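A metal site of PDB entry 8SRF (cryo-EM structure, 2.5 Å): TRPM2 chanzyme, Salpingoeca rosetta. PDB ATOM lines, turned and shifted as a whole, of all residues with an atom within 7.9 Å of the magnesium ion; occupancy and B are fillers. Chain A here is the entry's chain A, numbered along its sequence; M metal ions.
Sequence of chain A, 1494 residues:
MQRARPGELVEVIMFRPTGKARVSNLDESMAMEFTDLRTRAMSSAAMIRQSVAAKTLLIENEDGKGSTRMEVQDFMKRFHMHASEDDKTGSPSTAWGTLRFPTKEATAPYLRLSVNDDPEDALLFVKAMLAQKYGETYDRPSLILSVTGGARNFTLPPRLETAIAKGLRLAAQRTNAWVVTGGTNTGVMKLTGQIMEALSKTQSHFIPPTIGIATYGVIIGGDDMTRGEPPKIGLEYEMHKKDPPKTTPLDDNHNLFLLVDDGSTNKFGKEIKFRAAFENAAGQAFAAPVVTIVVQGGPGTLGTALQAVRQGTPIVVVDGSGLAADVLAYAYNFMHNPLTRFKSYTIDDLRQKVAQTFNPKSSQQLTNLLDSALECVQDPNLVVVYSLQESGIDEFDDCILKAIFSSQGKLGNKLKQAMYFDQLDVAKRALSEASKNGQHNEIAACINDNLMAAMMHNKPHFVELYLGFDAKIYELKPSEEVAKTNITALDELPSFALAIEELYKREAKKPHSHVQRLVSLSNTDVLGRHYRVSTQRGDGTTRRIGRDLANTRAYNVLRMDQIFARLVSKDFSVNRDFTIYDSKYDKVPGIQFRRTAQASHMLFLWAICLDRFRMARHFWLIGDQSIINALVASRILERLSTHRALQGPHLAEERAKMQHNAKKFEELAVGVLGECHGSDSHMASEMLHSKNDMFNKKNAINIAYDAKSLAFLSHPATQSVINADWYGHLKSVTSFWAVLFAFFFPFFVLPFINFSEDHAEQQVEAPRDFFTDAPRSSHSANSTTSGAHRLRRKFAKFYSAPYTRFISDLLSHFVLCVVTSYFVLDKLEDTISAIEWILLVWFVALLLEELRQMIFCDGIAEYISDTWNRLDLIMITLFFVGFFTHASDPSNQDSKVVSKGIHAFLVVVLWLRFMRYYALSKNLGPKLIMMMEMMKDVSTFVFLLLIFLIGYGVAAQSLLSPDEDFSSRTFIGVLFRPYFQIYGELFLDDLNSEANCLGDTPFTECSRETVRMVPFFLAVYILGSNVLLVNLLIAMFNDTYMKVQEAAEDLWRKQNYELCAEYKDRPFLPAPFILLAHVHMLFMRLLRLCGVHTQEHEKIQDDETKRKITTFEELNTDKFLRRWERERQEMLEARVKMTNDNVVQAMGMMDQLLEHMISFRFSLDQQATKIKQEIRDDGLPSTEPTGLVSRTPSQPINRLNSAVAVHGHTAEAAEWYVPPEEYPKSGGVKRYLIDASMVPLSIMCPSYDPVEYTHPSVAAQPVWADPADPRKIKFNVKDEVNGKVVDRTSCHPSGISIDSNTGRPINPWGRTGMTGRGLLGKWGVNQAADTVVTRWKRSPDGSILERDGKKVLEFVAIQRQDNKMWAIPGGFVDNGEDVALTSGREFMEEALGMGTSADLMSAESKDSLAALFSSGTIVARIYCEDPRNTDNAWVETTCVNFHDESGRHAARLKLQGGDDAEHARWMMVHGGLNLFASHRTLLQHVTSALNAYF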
ATOM      1  N   PHE A 593       3.604 -12.653  12.400  1.00  0.00           N
ATOM      2  CA  PHE A 593       3.034 -13.936  12.800  1.00  0.00           C
ATOM      3  C   PHE A 593       4.097 -14.867  13.363  1.00  0.00           C
ATOM      4  O   PHE A 593       3.809 -15.571  14.335  1.00  0.00           O
ATOM      5  CB  PHE A 593       2.320 -14.557  11.592  1.00  0.00           C
ATOM      6  CG  PHE A 593       1.789 -15.926  11.837  1.00  0.00           C
ATOM      7  CD1 PHE A 593       0.829 -16.149  12.852  1.00  0.00           C
ATOM      8  CD2 PHE A 593       2.208 -17.001  11.039  1.00  0.00           C
ATOM      9  CE1 PHE A 593       0.315 -17.430  13.076  1.00  0.00           C
ATOM     10  CE2 PHE A 593       1.706 -18.289  11.245  1.00  0.00           C
ATOM     11  CZ  PHE A 593       0.752 -18.500  12.266  1.00  0.00           C
ATOM     12  N   ALA A 597       4.378 -16.313  17.017  1.00  0.00           N
ATOM     13  CA  ALA A 597       4.215 -17.760  17.125  1.00  0.00           C
ATOM     14  C   ALA A 597       5.323 -18.375  17.978  1.00  0.00           C
ATOM     15  O   ALA A 597       5.034 -19.189  18.872  1.00  0.00           O
ATOM     16  CB  ALA A 597       4.190 -18.401  15.737  1.00  0.00           C
ATOM     17  N   SER A 600       5.120 -16.934  21.709  1.00  0.00           N
ATOM     18  CA  SER A 600       3.971 -17.626  22.315  1.00  0.00           C
ATOM     19  C   SER A 600       4.322 -19.053  22.686  1.00  0.00           C
ATOM     20  O   SER A 600       3.814 -19.545  23.693  1.00  0.00           O
ATOM     21  CB  SER A 600       2.791 -17.623  21.370  1.00  0.00           C
ATOM     22  OG  SER A 600       3.120 -18.407  20.276  1.00  0.00           O
ATOM     23  N   HIS A 618      -4.248 -19.946  26.502  1.00  0.00           N
ATOM     24  CA  HIS A 618      -4.192 -18.642  25.824  1.00  0.00           C
ATOM     25  C   HIS A 618      -2.969 -18.515  24.900  1.00  0.00           C
ATOM     26  O   HIS A 618      -3.111 -18.031  23.757  1.00  0.00           O
ATOM     27  CB  HIS A 618      -4.240 -17.485  26.805  1.00  0.00           C
ATOM     28  CG  HIS A 618      -4.291 -16.156  26.119  1.00  0.00           C
ATOM     29  ND1 HIS A 618      -5.391 -15.742  25.408  1.00  0.00           N
ATOM     30  CD2 HIS A 618      -3.363 -15.179  25.986  1.00  0.00           C
ATOM     31  CE1 HIS A 618      -5.158 -14.556  24.874  1.00  0.00           C
ATOM     32  NE2 HIS A 618      -3.939 -14.191  25.215  1.00  0.00           N
ATOM     33  N   PHE A 619      -1.778 -18.946  25.382  1.00  0.00           N
ATOM     34  CA  PHE A 619      -0.573 -18.920  24.545  1.00  0.00           C
ATOM     35  C   PHE A 619      -0.628 -19.962  23.436  1.00  0.00           C
ATOM     36  O   PHE A 619       0.014 -19.786  22.399  1.00  0.00           O
ATOM     37  CB  PHE A 619       0.730 -19.071  25.335  1.00  0.00           C
ATOM     38  CG  PHE A 619       1.029 -17.930  26.272  1.00  0.00           C
ATOM     39  CD1 PHE A 619       0.956 -16.615  25.791  1.00  0.00           C
ATOM     40  CD2 PHE A 619       1.545 -18.164  27.551  1.00  0.00           C
ATOM     41  CE1 PHE A 619       1.261 -15.529  26.618  1.00  0.00           C
ATOM     42  CE2 PHE A 619       1.867 -17.095  28.396  1.00  0.00           C
ATOM     43  CZ  PHE A 619       1.719 -15.778  27.920  1.00  0.00           C
ATOM     44  N   TRP A 620      -1.301 -21.088  23.693  1.00  0.00           N
ATOM     45  CA  TRP A 620      -1.575 -22.107  22.688  1.00  0.00           C
ATOM     46  C   TRP A 620      -2.489 -21.567  21.593  1.00  0.00           C
ATOM     47  O   TRP A 620      -2.304 -21.888  20.412  1.00  0.00           O
ATOM     48  CB  TRP A 620      -2.178 -23.329  23.382  1.00  0.00           C
ATOM     49  CG  TRP A 620      -2.751 -24.374  22.474  1.00  0.00           C
ATOM     50  CD1 TRP A 620      -2.051 -25.325  21.795  1.00  0.00           C
ATOM     51  CD2 TRP A 620      -4.124 -24.583  22.157  1.00  0.00           C
ATOM     52  NE1 TRP A 620      -2.904 -26.117  21.068  1.00  0.00           N
ATOM     53  CE2 TRP A 620      -4.193 -25.680  21.273  1.00  0.00           C
ATOM     54  CE3 TRP A 620      -5.322 -23.936  22.532  1.00  0.00           C
ATOM     55  CZ2 TRP A 620      -5.401 -26.158  20.755  1.00  0.00           C
ATOM     56  CZ3 TRP A 620      -6.522 -24.411  22.019  1.00  0.00           C
ATOM     57  CH2 TRP A 620      -6.545 -25.508  21.137  1.00  0.00           C
ATOM     58  N   LEU A 621      -3.519 -20.776  21.970  1.00  0.00           N
ATOM     59  CA  LEU A 621      -4.426 -20.178  20.983  1.00  0.00           C
ATOM     60  C   LEU A 621      -3.801 -19.096  20.102  1.00  0.00           C
ATOM     61  O   LEU A 621      -4.143 -19.030  18.911  1.00  0.00           O
ATOM     62  CB  LEU A 621      -5.642 -19.606  21.737  1.00  0.00           C
ATOM     63  CG  LEU A 621      -6.713 -18.713  21.083  1.00  0.00           C
ATOM     64  CD1 LEU A 621      -7.425 -19.304  19.881  1.00  0.00           C
ATOM     65  CD2 LEU A 621      -7.725 -18.281  22.143  1.00  0.00           C
ATOM     66  N   ILE A 622      -2.958 -18.205  20.668  1.00  0.00           N
ATOM     67  CA  ILE A 622      -2.317 -17.153  19.849  1.00  0.00           C
ATOM     68  C   ILE A 622      -1.311 -17.681  18.813  1.00  0.00           C
ATOM     69  O   ILE A 622      -1.322 -17.206  17.671  1.00  0.00           O
ATOM     70  CB  ILE A 622      -1.744 -15.970  20.666  1.00  0.00           C
ATOM     71  CG1 ILE A 622      -0.769 -16.380  21.749  1.00  0.00           C
ATOM     72  CG2 ILE A 622      -2.929 -15.132  21.210  1.00  0.00           C
ATOM     73  CD1 ILE A 622      -0.244 -15.230  22.581  1.00  0.00           C
ATOM     74  N   GLY A 623      -0.468 -18.647  19.180  1.00  0.00           N
ATOM     75  CA  GLY A 623       0.536 -19.204  18.300  1.00  0.00           C
ATOM     76  C   GLY A 623      -0.006 -20.206  17.302  1.00  0.00           C
ATOM     77  O   GLY A 623      -1.209 -20.368  17.121  1.00  0.00           O
ATOM     78  N   ASP A 624       0.920 -20.916  16.651  1.00  0.00           N
ATOM     79  CA  ASP A 624       0.498 -21.900  15.663  1.00  0.00           C
ATOM     80  C   ASP A 624       0.862 -23.316  16.089  1.00  0.00           C
ATOM     81  O   ASP A 624       1.409 -23.522  17.183  1.00  0.00           O
ATOM     82  CB  ASP A 624       1.064 -21.540  14.284  1.00  0.00           C
ATOM     83  CG  ASP A 624       2.579 -21.779  14.123  1.00  0.00           C
ATOM     84  OD1 ASP A 624       3.383 -21.680  15.089  1.00  0.00           O
ATOM     85  OD2 ASP A 624       2.985 -22.089  12.984  1.00  0.00           O
ATOM     86  N   GLN A 625       0.576 -24.247  15.151  1.00  0.00           N
ATOM     87  CA  GLN A 625       0.753 -25.703  15.248  1.00  0.00           C
ATOM     88  C   GLN A 625       0.003 -26.255  16.469  1.00  0.00           C
ATOM     89  O   GLN A 625       0.606 -26.901  17.328  1.00  0.00           O
ATOM     90  CB  GLN A 625       2.237 -26.124  15.268  1.00  0.00           C
ATOM     91  CG  GLN A 625       2.912 -26.068  13.916  1.00  0.00           C
ATOM     92  CD  GLN A 625       2.300 -27.026  12.921  1.00  0.00           C
ATOM     93  OE1 GLN A 625       2.006 -28.176  13.244  1.00  0.00           O
ATOM     94  NE2 GLN A 625       2.106 -26.551  11.690  1.00  0.00           N
ATOM     95  N   SER A 626      -1.319 -25.963  16.503  1.00  0.00           N
ATOM     96  CA  SER A 626      -2.217 -26.135  17.654  1.00  0.00           C
ATOM     97  C   SER A 626      -2.363 -27.585  18.118  1.00  0.00           C
ATOM     98  O   SER A 626      -2.371 -27.851  19.335  1.00  0.00           O
ATOM     99  CB  SER A 626      -3.597 -25.550  17.317  1.00  0.00           C
ATOM    100  OG  SER A 626      -3.511 -24.183  16.966  1.00  0.00           O
ATOM    101  N   THR A1110      -1.438 -24.673   7.286  1.00  0.00           N
ATOM    102  CA  THR A1110      -1.284 -23.816   8.474  1.00  0.00           C
ATOM    103  C   THR A1110      -2.483 -22.873   8.682  1.00  0.00           C
ATOM    104  O   THR A1110      -3.020 -22.780   9.802  1.00  0.00           O
ATOM    105  CB  THR A1110       0.033 -23.033   8.333  1.00  0.00           C
ATOM    106  OG1 THR A1110       1.130 -23.950   8.351  1.00  0.00           O
ATOM    107  CG2 THR A1110       0.241 -22.015   9.452  1.00  0.00           C
ATOM    108  N   GLU A1113      -5.589 -25.018   9.581  1.00  0.00           N
ATOM    109  CA  GLU A1113      -5.492 -25.473  10.971  1.00  0.00           C
ATOM    110  C   GLU A1113      -5.831 -24.356  11.959  1.00  0.00           C
ATOM    111  O   GLU A1113      -6.526 -24.605  12.953  1.00  0.00           O
ATOM    112  CB  GLU A1113      -4.078 -26.024  11.217  1.00  0.00           C
ATOM    113  CG  GLU A1113      -3.801 -26.559  12.611  1.00  0.00           C
ATOM    114  CD  GLU A1113      -2.440 -27.221  12.727  1.00  0.00           C
ATOM    115  OE1 GLU A1113      -1.586 -26.969  11.843  1.00  0.00           O
ATOM    116  OE2 GLU A1113      -2.217 -27.975  13.693  1.00  0.00           O
ATOM    117  N   GLU A1114      -5.359 -23.114  11.681  1.00  0.00           N
ATOM    118  CA  GLU A1114      -5.666 -21.941  12.513  1.00  0.00           C
ATOM    119  C   GLU A1114      -7.142 -21.558  12.455  1.00  0.00           C
ATOM    120  O   GLU A1114      -7.717 -21.193  13.500  1.00  0.00           O
ATOM    121  CB  GLU A1114      -4.777 -20.748  12.166  1.00  0.00           C
ATOM    122  CG  GLU A1114      -3.394 -20.998  12.635  1.00  0.00           C
ATOM    123  CD  GLU A1114      -3.328 -20.858  14.140  1.00  0.00           C
ATOM    124  OE1 GLU A1114      -3.984 -19.964  14.706  1.00  0.00           O
ATOM    125  OE2 GLU A1114      -2.754 -21.748  14.777  1.00  0.00           O
ATOM    126  N   LEU A1115      -7.730 -21.592  11.238  1.00  0.00           N
ATOM    127  CA  LEU A1115      -9.147 -21.300  11.012  1.00  0.00           C
ATOM    128  C   LEU A1115     -10.037 -22.316  11.737  1.00  0.00           C
ATOM    129  O   LEU A1115     -11.001 -21.925  12.412  1.00  0.00           O
ATOM    130  CB  LEU A1115      -9.445 -21.301   9.510  1.00  0.00           C
ATOM    131  CG  LEU A1115     -10.893 -21.079   9.081  1.00  0.00           C
ATOM    132  CD1 LEU A1115     -11.247 -19.612   9.143  1.00  0.00           C
ATOM    133  CD2 LEU A1115     -11.136 -21.638   7.692  1.00  0.00           C
ATOM    134  N   THR A1117      -9.046 -24.166  14.332  1.00  0.00           N
ATOM    135  CA  THR A1117      -8.789 -23.945  15.760  1.00  0.00           C
ATOM    136  C   THR A1117      -9.729 -22.884  16.327  1.00  0.00           C
ATOM    137  O   THR A1117     -10.322 -23.081  17.410  1.00  0.00           O
ATOM    138  CB  THR A1117      -7.328 -23.555  15.961  1.00  0.00           C
ATOM    139  OG1 THR A1117      -6.485 -24.546  15.353  1.00  0.00           O
ATOM    140  CG2 THR A1117      -6.963 -23.464  17.436  1.00  0.00           C
ATOM    141  N   ASP A1118      -9.856 -21.746  15.600  1.00  0.00           N
ATOM    142  CA  ASP A1118     -10.785 -20.661  15.958  1.00  0.00           C
ATOM    143  C   ASP A1118     -12.247 -21.121  15.905  1.00  0.00           C
ATOM    144  O   ASP A1118     -13.050 -20.720  16.763  1.00  0.00           O
ATOM    145  CB  ASP A1118     -10.594 -19.428  15.076  1.00  0.00           C
ATOM    146  CG  ASP A1118      -9.199 -18.853  15.159  1.00  0.00           C
ATOM    147  OD1 ASP A1118      -8.679 -18.707  16.290  1.00  0.00           O
ATOM    148  OD2 ASP A1118      -8.664 -18.445  14.118  1.00  0.00           O
HETATM  149 MG    MG M   1      -3.270 -19.886  16.716  1.00  0.00          MG
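The side-chain hydroxyl (OG) of Ser 626 sits at hydrogen-bond distance from the side-chain carboxylate (OE2) of Glu 1114 (3.4 Å).
Residues that only touch the magnesium ion: Ile 622. The nearest printed residue that does not touch the magnesium ion is Ser 626 (4.3 Å).
The magnesium ion is bound by the side-chain carboxylate (OE1) of Glu 1114 (2.1 Å), the backbone carbonyl oxygen (O) of Gly 623 (2.2 Å) and the backbone carbonyl oxygen (O) of Leu 621 (2.5 Å). Slightly farther from the magnesium ion lies the side-chain carboxylate (OE2) of Glu 1114 (2.7 Å).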
